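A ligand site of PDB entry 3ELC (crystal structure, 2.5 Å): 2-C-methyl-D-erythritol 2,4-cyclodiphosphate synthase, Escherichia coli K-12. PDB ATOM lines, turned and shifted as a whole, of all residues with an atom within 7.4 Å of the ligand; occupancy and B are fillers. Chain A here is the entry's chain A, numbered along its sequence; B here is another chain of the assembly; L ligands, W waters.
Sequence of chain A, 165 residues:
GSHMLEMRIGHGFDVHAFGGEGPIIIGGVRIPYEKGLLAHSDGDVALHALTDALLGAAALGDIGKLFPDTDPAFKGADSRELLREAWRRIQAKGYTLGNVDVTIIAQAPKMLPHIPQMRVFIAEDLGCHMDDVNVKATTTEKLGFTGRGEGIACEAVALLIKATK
Water W1 lies within hydrogen-bond range of N of Ala 137, OD2 of Asp 62 of chain B and O5 of the ligand.
O of Thr 138 sits close to F1 of the ligand (3.2 Å). The backbone NH (N) of Thr 139 lies close to a fluorine (F1) of the ligand (3.1 Å). Lys 110 touches the ligand (CG to O1, 3.4 Å). Ala 137 touches the ligand. Gly 64 of chain B touches the ligand (CA to O4, 3.4 Å). Of the 27 residues printed, 10 come within 4 Å of the ligand.
OD1 of Asp 62 of chain B sits close to N of Gly 64 of chain B (3.4 Å). The backbone carbonyl oxygen of Ile 104 lies within hydrogen-bond range of the backbone NH of Thr 138, at 3.0 Å. O of Thr 138 lies within hydrogen-bond range of N of Ala 106, at 3.2 Å. OD1 of Asp 62 of chain B is in hydrogen-bond range of N of Lys 65 of chain B (3.4 Å). The backbone NH (N) of Glu 141 lies close to the side-chain hydroxyl (OG1) of Thr 139 (3.4 Å).
N2 of the ligand is in hydrogen-bond range of O of Ala 106. A nitrogen (N2) of the ligand is in hydrogen-bond range of the backbone carbonyl oxygen of Pro 109 (3.0 Å). The side-chain carboxylate (OD2) of Asp 62 of chain B is in hydrogen-bond range of an oxygen (O4) of the ligand, 2.9 Å away. N of Leu 112 is in hydrogen-bond range of O1 of the ligand (2.9 Å). O1 of the ligand sits at hydrogen-bond distance from N of Met 111 (2.7 Å).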
ATOM      1  N   ILE A 104     -17.168 -22.818 -25.286  1.00  0.00           N
ATOM      2  CA  ILE A 104     -15.764 -23.036 -25.416  1.00  0.00           C
ATOM      3  C   ILE A 104     -15.557 -24.175 -26.422  1.00  0.00           C
ATOM      4  O   ILE A 104     -16.280 -25.172 -26.412  1.00  0.00           O
ATOM      5  CB  ILE A 104     -15.189 -23.372 -24.024  1.00  0.00           C
ATOM      6  CG1 ILE A 104     -15.691 -22.328 -22.984  1.00  0.00           C
ATOM      7  CG2 ILE A 104     -13.661 -23.447 -24.055  1.00  0.00           C
ATOM      8  CD1 ILE A 104     -15.361 -22.664 -21.477  1.00  0.00           C
ATOM      9  N   ILE A 105     -14.585 -24.013 -27.315  1.00  0.00           N
ATOM     10  CA  ILE A 105     -14.334 -25.008 -28.359  1.00  0.00           C
ATOM     11  C   ILE A 105     -12.865 -25.415 -28.283  1.00  0.00           C
ATOM     12  O   ILE A 105     -11.992 -24.691 -28.734  1.00  0.00           O
ATOM     13  CB  ILE A 105     -14.704 -24.498 -29.796  1.00  0.00           C
ATOM     14  CG1 ILE A 105     -16.088 -23.816 -29.807  1.00  0.00           C
ATOM     15  CG2 ILE A 105     -14.695 -25.634 -30.793  1.00  0.00           C
ATOM     16  CD1 ILE A 105     -16.416 -23.041 -31.103  1.00  0.00           C
ATOM     17  N   ALA A 106     -12.608 -26.560 -27.693  1.00  0.00           N
ATOM     18  CA  ALA A 106     -11.286 -26.950 -27.285  1.00  0.00           C
ATOM     19  C   ALA A 106     -11.236 -28.460 -27.351  1.00  0.00           C
ATOM     20  O   ALA A 106     -12.159 -29.140 -26.866  1.00  0.00           O
ATOM     21  CB  ALA A 106     -11.007 -26.476 -25.850  1.00  0.00           C
ATOM     22  N   GLN A 107     -10.178 -28.990 -27.973  1.00  0.00           N
ATOM     23  CA  GLN A 107      -9.956 -30.422 -27.971  1.00  0.00           C
ATOM     24  C   GLN A 107      -9.526 -30.832 -26.563  1.00  0.00           C
ATOM     25  O   GLN A 107      -9.868 -31.913 -26.089  1.00  0.00           O
ATOM     26  CB  GLN A 107      -8.914 -30.827 -29.007  1.00  0.00           C
ATOM     27  CG  GLN A 107      -8.824 -32.309 -29.244  1.00  0.00           C
ATOM     28  CD  GLN A 107     -10.089 -32.887 -29.840  1.00  0.00           C
ATOM     29  OE1 GLN A 107     -10.694 -32.316 -30.751  1.00  0.00           O
ATOM     30  NE2 GLN A 107     -10.510 -34.027 -29.327  1.00  0.00           N
ATOM     31  N   ALA A 108      -8.812 -29.935 -25.906  1.00  0.00           N
ATOM     32  CA  ALA A 108      -8.226 -30.154 -24.595  1.00  0.00           C
ATOM     33  C   ALA A 108      -7.793 -28.797 -24.058  1.00  0.00           C
ATOM     34  O   ALA A 108      -7.527 -27.884 -24.841  1.00  0.00           O
ATOM     35  CB  ALA A 108      -7.036 -31.077 -24.711  1.00  0.00           C
ATOM     36  N   PRO A 109      -7.694 -28.642 -22.726  1.00  0.00           N
ATOM     37  CA  PRO A 109      -8.005 -29.635 -21.692  1.00  0.00           C
ATOM     38  C   PRO A 109      -9.470 -29.697 -21.403  1.00  0.00           C
ATOM     39  O   PRO A 109     -10.268 -28.983 -22.021  1.00  0.00           O
ATOM     40  CB  PRO A 109      -7.279 -29.073 -20.479  1.00  0.00           C
ATOM     41  CG  PRO A 109      -7.373 -27.589 -20.637  1.00  0.00           C
ATOM     42  CD  PRO A 109      -7.187 -27.384 -22.135  1.00  0.00           C
ATOM     43  N   LYS A 110      -9.812 -30.553 -20.431  1.00  0.00           N
ATOM     44  CA  LYS A 110     -11.156 -30.717 -19.884  1.00  0.00           C
ATOM     45  C   LYS A 110     -11.600 -29.432 -19.171  1.00  0.00           C
ATOM     46  O   LYS A 110     -10.900 -28.929 -18.297  1.00  0.00           O
ATOM     47  CB  LYS A 110     -11.134 -31.902 -18.900  1.00  0.00           C
ATOM     48  CG  LYS A 110     -12.448 -32.645 -18.722  1.00  0.00           C
ATOM     49  CD  LYS A 110     -12.556 -33.835 -19.667  1.00  0.00           C
ATOM     50  CE  LYS A 110     -14.017 -34.037 -20.113  1.00  0.00           C
ATOM     51  NZ  LYS A 110     -14.158 -34.877 -21.373  1.00  0.00           N
ATOM     52  N   MET A 111     -12.767 -28.914 -19.524  1.00  0.00           N
ATOM     53  CA  MET A 111     -13.246 -27.643 -19.007  1.00  0.00           C
ATOM     54  C   MET A 111     -14.213 -27.798 -17.823  1.00  0.00           C
ATOM     55  O   MET A 111     -14.256 -26.938 -16.948  1.00  0.00           O
ATOM     56  CB  MET A 111     -13.884 -26.797 -20.132  1.00  0.00           C
ATOM     57  CG  MET A 111     -12.933 -26.431 -21.268  1.00  0.00           C
ATOM     58  SD  MET A 111     -11.660 -25.213 -20.881  1.00  0.00           S
ATOM     59  CE  MET A 111     -10.569 -25.314 -22.293  1.00  0.00           C
ATOM     60  N   LEU A 112     -14.976 -28.894 -17.833  1.00  0.00           N
ATOM     61  CA  LEU A 112     -15.843 -29.389 -16.734  1.00  0.00           C
ATOM     62  C   LEU A 112     -15.449 -29.093 -15.256  1.00  0.00           C
ATOM     63  O   LEU A 112     -16.267 -28.552 -14.499  1.00  0.00           O
ATOM     64  CB  LEU A 112     -16.032 -30.905 -16.878  1.00  0.00           C
ATOM     65  CG  LEU A 112     -16.947 -31.723 -15.943  1.00  0.00           C
ATOM     66  CD1 LEU A 112     -18.325 -31.896 -16.549  1.00  0.00           C
ATOM     67  CD2 LEU A 112     -16.371 -33.124 -15.619  1.00  0.00           C
ATOM     68  N   PRO A 113     -14.223 -29.454 -14.823  1.00  0.00           N
ATOM     69  CA  PRO A 113     -13.958 -29.205 -13.399  1.00  0.00           C
ATOM     70  C   PRO A 113     -14.109 -27.714 -13.088  1.00  0.00           C
ATOM     71  O   PRO A 113     -14.622 -27.341 -12.030  1.00  0.00           O
ATOM     72  CB  PRO A 113     -12.481 -29.594 -13.236  1.00  0.00           C
ATOM     73  CG  PRO A 113     -12.199 -30.539 -14.335  1.00  0.00           C
ATOM     74  CD  PRO A 113     -13.137 -30.222 -15.480  1.00  0.00           C
ATOM     75  N   HIS A 114     -13.686 -26.868 -14.039  1.00  0.00           N
ATOM     76  CA  HIS A 114     -13.477 -25.450 -13.811  1.00  0.00           C
ATOM     77  C   HIS A 114     -14.675 -24.580 -14.211  1.00  0.00           C
ATOM     78  O   HIS A 114     -14.696 -23.402 -13.906  1.00  0.00           O
ATOM     79  CB  HIS A 114     -12.210 -24.983 -14.560  1.00  0.00           C
ATOM     80  CG  HIS A 114     -11.016 -25.856 -14.329  1.00  0.00           C
ATOM     81  ND1 HIS A 114     -10.441 -26.627 -15.323  1.00  0.00           N
ATOM     82  CD2 HIS A 114     -10.300 -26.110 -13.207  1.00  0.00           C
ATOM     83  CE1 HIS A 114      -9.415 -27.298 -14.827  1.00  0.00           C
ATOM     84  NE2 HIS A 114      -9.305 -27.005 -13.547  1.00  0.00           N
ATOM     85  N   ILE A 115     -15.672 -25.166 -14.855  1.00  0.00           N
ATOM     86  CA  ILE A 115     -16.781 -24.402 -15.396  1.00  0.00           C
ATOM     87  C   ILE A 115     -17.593 -23.685 -14.309  1.00  0.00           C
ATOM     88  O   ILE A 115     -17.854 -22.497 -14.459  1.00  0.00           O
ATOM     89  CB  ILE A 115     -17.665 -25.239 -16.373  1.00  0.00           C
ATOM     90  CG1 ILE A 115     -17.064 -25.165 -17.792  1.00  0.00           C
ATOM     91  CG2 ILE A 115     -19.134 -24.759 -16.386  1.00  0.00           C
ATOM     92  CD1 ILE A 115     -17.640 -26.155 -18.800  1.00  0.00           C
ATOM     93  N   LYS A 136     -20.741 -23.747 -21.463  1.00  0.00           N
ATOM     94  CA  LYS A 136     -20.524 -25.141 -21.792  1.00  0.00           C
ATOM     95  C   LYS A 136     -19.232 -25.294 -22.614  1.00  0.00           C
ATOM     96  O   LYS A 136     -18.598 -24.306 -22.952  1.00  0.00           O
ATOM     97  CB  LYS A 136     -21.724 -25.669 -22.567  1.00  0.00           C
ATOM     98  CG  LYS A 136     -21.883 -25.041 -23.908  1.00  0.00           C
ATOM     99  CD  LYS A 136     -23.160 -25.466 -24.582  1.00  0.00           C
ATOM    100  CE  LYS A 136     -23.719 -24.347 -25.447  1.00  0.00           C
ATOM    101  NZ  LYS A 136     -24.607 -23.436 -24.689  1.00  0.00           N
ATOM    102  N   ALA A 137     -18.871 -26.525 -22.923  1.00  0.00           N
ATOM    103  CA  ALA A 137     -17.646 -26.816 -23.646  1.00  0.00           C
ATOM    104  C   ALA A 137     -17.897 -27.968 -24.630  1.00  0.00           C
ATOM    105  O   ALA A 137     -18.708 -28.834 -24.329  1.00  0.00           O
ATOM    106  CB  ALA A 137     -16.557 -27.198 -22.682  1.00  0.00           C
ATOM    107  N   THR A 138     -17.238 -27.947 -25.781  1.00  0.00           N
ATOM    108  CA  THR A 138     -17.362 -29.013 -26.776  1.00  0.00           C
ATOM    109  C   THR A 138     -16.100 -29.192 -27.676  1.00  0.00           C
ATOM    110  O   THR A 138     -15.328 -28.251 -27.837  1.00  0.00           O
ATOM    111  CB  THR A 138     -18.627 -28.830 -27.635  1.00  0.00           C
ATOM    112  OG1 THR A 138     -18.835 -29.999 -28.434  1.00  0.00           O
ATOM    113  CG2 THR A 138     -18.538 -27.614 -28.567  1.00  0.00           C
ATOM    114  N   THR A 139     -15.876 -30.383 -28.238  1.00  0.00           N
ATOM    115  CA  THR A 139     -14.779 -30.576 -29.208  1.00  0.00           C
ATOM    116  C   THR A 139     -15.203 -30.494 -30.664  1.00  0.00           C
ATOM    117  O   THR A 139     -16.389 -30.555 -30.978  1.00  0.00           O
ATOM    118  CB  THR A 139     -14.074 -31.954 -29.063  1.00  0.00           C
ATOM    119  OG1 THR A 139     -15.046 -33.012 -29.182  1.00  0.00           O
ATOM    120  CG2 THR A 139     -13.328 -32.067 -27.759  1.00  0.00           C
ATOM    121  N   THR A 140     -14.218 -30.395 -31.543  1.00  0.00           N
ATOM    122  CA  THR A 140     -14.441 -30.568 -32.975  1.00  0.00           C
ATOM    123  C   THR A 140     -14.049 -31.977 -33.408  1.00  0.00           C
ATOM    124  O   THR A 140     -13.808 -32.196 -34.576  1.00  0.00           O
ATOM    125  CB  THR A 140     -13.633 -29.549 -33.807  1.00  0.00           C
ATOM    126  OG1 THR A 140     -12.271 -29.588 -33.427  1.00  0.00           O
ATOM    127  CG2 THR A 140     -14.158 -28.132 -33.586  1.00  0.00           C
ATOM    128  N   GLU A 141     -14.002 -32.931 -32.459  1.00  0.00           N
ATOM    129  CA  GLU A 141     -13.711 -34.356 -32.727  1.00  0.00           C
ATOM    130  C   GLU A 141     -12.449 -34.604 -33.551  1.00  0.00           C
ATOM    131  O   GLU A 141     -12.455 -35.419 -34.472  1.00  0.00           O
ATOM    132  CB  GLU A 141     -14.878 -35.058 -33.440  1.00  0.00           C
ATOM    133  CG  GLU A 141     -16.276 -34.927 -32.808  1.00  0.00           C
ATOM    134  CD  GLU A 141     -16.516 -35.827 -31.599  1.00  0.00           C
ATOM    135  OE1 GLU A 141     -17.552 -35.616 -30.902  1.00  0.00           O
ATOM    136  OE2 GLU A 141     -15.675 -36.710 -31.311  1.00  0.00           O
ATOM    137  N   ILE A 152      -7.640 -22.721 -29.276  1.00  0.00           N
ATOM    138  CA  ILE A 152      -8.937 -22.763 -28.610  1.00  0.00           C
ATOM    139  C   ILE A 152      -9.803 -21.687 -29.221  1.00  0.00           C
ATOM    140  O   ILE A 152      -9.395 -20.537 -29.353  1.00  0.00           O
ATOM    141  CB  ILE A 152      -8.788 -22.569 -27.069  1.00  0.00           C
ATOM    142  CG1 ILE A 152      -8.071 -23.783 -26.477  1.00  0.00           C
ATOM    143  CG2 ILE A 152     -10.172 -22.316 -26.415  1.00  0.00           C
ATOM    144  CD1 ILE A 152      -8.150 -23.939 -24.986  1.00  0.00           C
ATOM    145  N   ASP B  14     -22.015 -28.148 -32.598  1.00  0.00           N
ATOM    146  CA  ASP B  14     -21.565 -29.540 -32.554  1.00  0.00           C
ATOM    147  C   ASP B  14     -20.896 -29.904 -33.880  1.00  0.00           C
ATOM    148  O   ASP B  14     -21.215 -29.315 -34.923  1.00  0.00           O
ATOM    149  CB  ASP B  14     -22.733 -30.502 -32.259  1.00  0.00           C
ATOM    150  CG  ASP B  14     -22.270 -31.913 -31.878  1.00  0.00           C
ATOM    151  OD1 ASP B  14     -21.326 -32.069 -31.070  1.00  0.00           O
ATOM    152  OD2 ASP B  14     -22.892 -32.880 -32.345  1.00  0.00           O
ATOM    153  N   ASP B  52     -28.417 -28.153 -27.087  1.00  0.00           N
ATOM    154  CA  ASP B  52     -27.469 -27.347 -26.312  1.00  0.00           C
ATOM    155  C   ASP B  52     -27.865 -25.877 -26.263  1.00  0.00           C
ATOM    156  O   ASP B  52     -27.573 -25.189 -25.299  1.00  0.00           O
ATOM    157  CB  ASP B  52     -26.036 -27.506 -26.869  1.00  0.00           C
ATOM    158  CG  ASP B  52     -25.307 -28.752 -26.322  1.00  0.00           C
ATOM    159  OD1 ASP B  52     -25.719 -29.299 -25.280  1.00  0.00           O
ATOM    160  OD2 ASP B  52     -24.307 -29.198 -26.922  1.00  0.00           O
ATOM    161  N   GLY B  61     -26.725 -26.092 -18.515  1.00  0.00           N
ATOM    162  CA  GLY B  61     -25.466 -26.689 -18.964  1.00  0.00           C
ATOM    163  C   GLY B  61     -25.456 -27.066 -20.445  1.00  0.00           C
ATOM    164  O   GLY B  61     -25.652 -26.231 -21.304  1.00  0.00           O
ATOM    165  N   ASP B  62     -25.199 -28.340 -20.707  1.00  0.00           N
ATOM    166  CA  ASP B  62     -25.318 -28.918 -22.043  1.00  0.00           C
ATOM    167  C   ASP B  62     -25.712 -30.383 -21.930  1.00  0.00           C
ATOM    168  O   ASP B  62     -25.989 -30.847 -20.822  1.00  0.00           O
ATOM    169  CB  ASP B  62     -24.020 -28.726 -22.845  1.00  0.00           C
ATOM    170  CG  ASP B  62     -22.830 -29.457 -22.243  1.00  0.00           C
ATOM    171  OD1 ASP B  62     -22.914 -30.034 -21.138  1.00  0.00           O
ATOM    172  OD2 ASP B  62     -21.776 -29.437 -22.906  1.00  0.00           O
ATOM    173  N   ILE B  63     -25.761 -31.113 -23.048  1.00  0.00           N
ATOM    174  CA  ILE B  63     -26.138 -32.530 -22.992  1.00  0.00           C
ATOM    175  C   ILE B  63     -25.276 -33.331 -22.017  1.00  0.00           C
ATOM    176  O   ILE B  63     -25.811 -34.093 -21.218  1.00  0.00           O
ATOM    177  CB  ILE B  63     -26.164 -33.232 -24.392  1.00  0.00           C
ATOM    178  CG1 ILE B  63     -24.747 -33.512 -24.956  1.00  0.00           C
ATOM    179  CG2 ILE B  63     -27.135 -32.530 -25.359  1.00  0.00           C
ATOM    180  CD1 ILE B  63     -23.749 -32.262 -25.155  1.00  0.00           C
ATOM    181  N   GLY B  64     -23.955 -33.134 -22.050  1.00  0.00           N
ATOM    182  CA  GLY B  64     -23.043 -33.808 -21.136  1.00  0.00           C
ATOM    183  C   GLY B  64     -23.437 -33.696 -19.663  1.00  0.00           C
ATOM    184  O   GLY B  64     -23.038 -34.534 -18.847  1.00  0.00           O
ATOM    185  N   LYS B  65     -24.202 -32.651 -19.335  1.00  0.00           N
ATOM    186  CA  LYS B  65     -24.597 -32.366 -17.951  1.00  0.00           C
ATOM    187  C   LYS B  65     -25.997 -32.879 -17.587  1.00  0.00           C
ATOM    188  O   LYS B  65     -26.283 -33.076 -16.407  1.00  0.00           O
ATOM    189  CB  LYS B  65     -24.497 -30.878 -17.660  1.00  0.00           C
ATOM    190  CG  LYS B  65     -24.438 -30.522 -16.171  1.00  0.00           C
ATOM    191  CD  LYS B  65     -23.754 -29.161 -15.963  1.00  0.00           C
ATOM    192  CE  LYS B  65     -23.372 -28.898 -14.509  1.00  0.00           C
ATOM    193  NZ  LYS B  65     -24.513 -28.286 -13.746  1.00  0.00           N
ATOM    194  N   ASP B  69     -22.260 -40.031 -18.344  1.00  0.00           N
ATOM    195  CA  ASP B  69     -21.923 -41.451 -18.498  1.00  0.00           C
ATOM    196  C   ASP B  69     -22.337 -42.349 -17.302  1.00  0.00           C
ATOM    197  O   ASP B  69     -22.404 -43.569 -17.430  1.00  0.00           O
ATOM    198  CB  ASP B  69     -20.431 -41.627 -18.806  1.00  0.00           C
ATOM    199  CG  ASP B  69     -20.001 -40.866 -20.069  1.00  0.00           C
ATOM    200  OD1 ASP B  69     -20.363 -41.306 -21.193  1.00  0.00           O
ATOM    201  OD2 ASP B  69     -19.295 -39.829 -19.942  1.00  0.00           O
HETATM  202  O1  LIG L   1     -14.775 -30.624 -20.116  1.00  0.00           O
HETATM  203  C1  LIG L   1     -14.773 -30.560 -21.348  1.00  0.00           C
HETATM  204  N1  LIG L   1     -13.709 -29.929 -21.975  1.00  0.00           N
HETATM  205  C2  LIG L   1     -13.665 -29.831 -23.335  1.00  0.00           C
HETATM  206  N2  LIG L   1     -12.634 -29.214 -23.890  1.00  0.00           N
HETATM  207  C3  LIG L   1     -14.675 -30.367 -24.108  1.00  0.00           C
HETATM  208  F1  LIG L   1     -14.606 -30.232 -25.443  1.00  0.00           F
HETATM  209  C4  LIG L   1     -15.755 -31.006 -23.523  1.00  0.00           C
HETATM  210  N3  LIG L   1     -15.822 -31.121 -22.113  1.00  0.00           N
HETATM  211  C5  LIG L   1     -16.955 -31.820 -21.446  1.00  0.00           C
HETATM  212  O2  LIG L   1     -17.082 -33.022 -22.254  1.00  0.00           O
HETATM  213  C6  LIG L   1     -18.489 -33.239 -22.479  1.00  0.00           C
HETATM  214  C7  LIG L   1     -18.660 -33.925 -23.848  1.00  0.00           C
HETATM  215  O3  LIG L   1     -18.214 -33.062 -24.931  1.00  0.00           O
HETATM  216  C8  LIG L   1     -19.082 -31.846 -22.543  1.00  0.00           C
HETATM  217  O4  LIG L   1     -20.458 -31.891 -22.233  1.00  0.00           O
HETATM  218  C9  LIG L   1     -18.311 -31.102 -21.466  1.00  0.00           C
HETATM  219  O5  LIG L   1     -18.948 -31.295 -20.213  1.00  0.00           O
HETATM  220  O   HOH W   1     -19.785 -28.337 -20.934  1.00  0.00           O
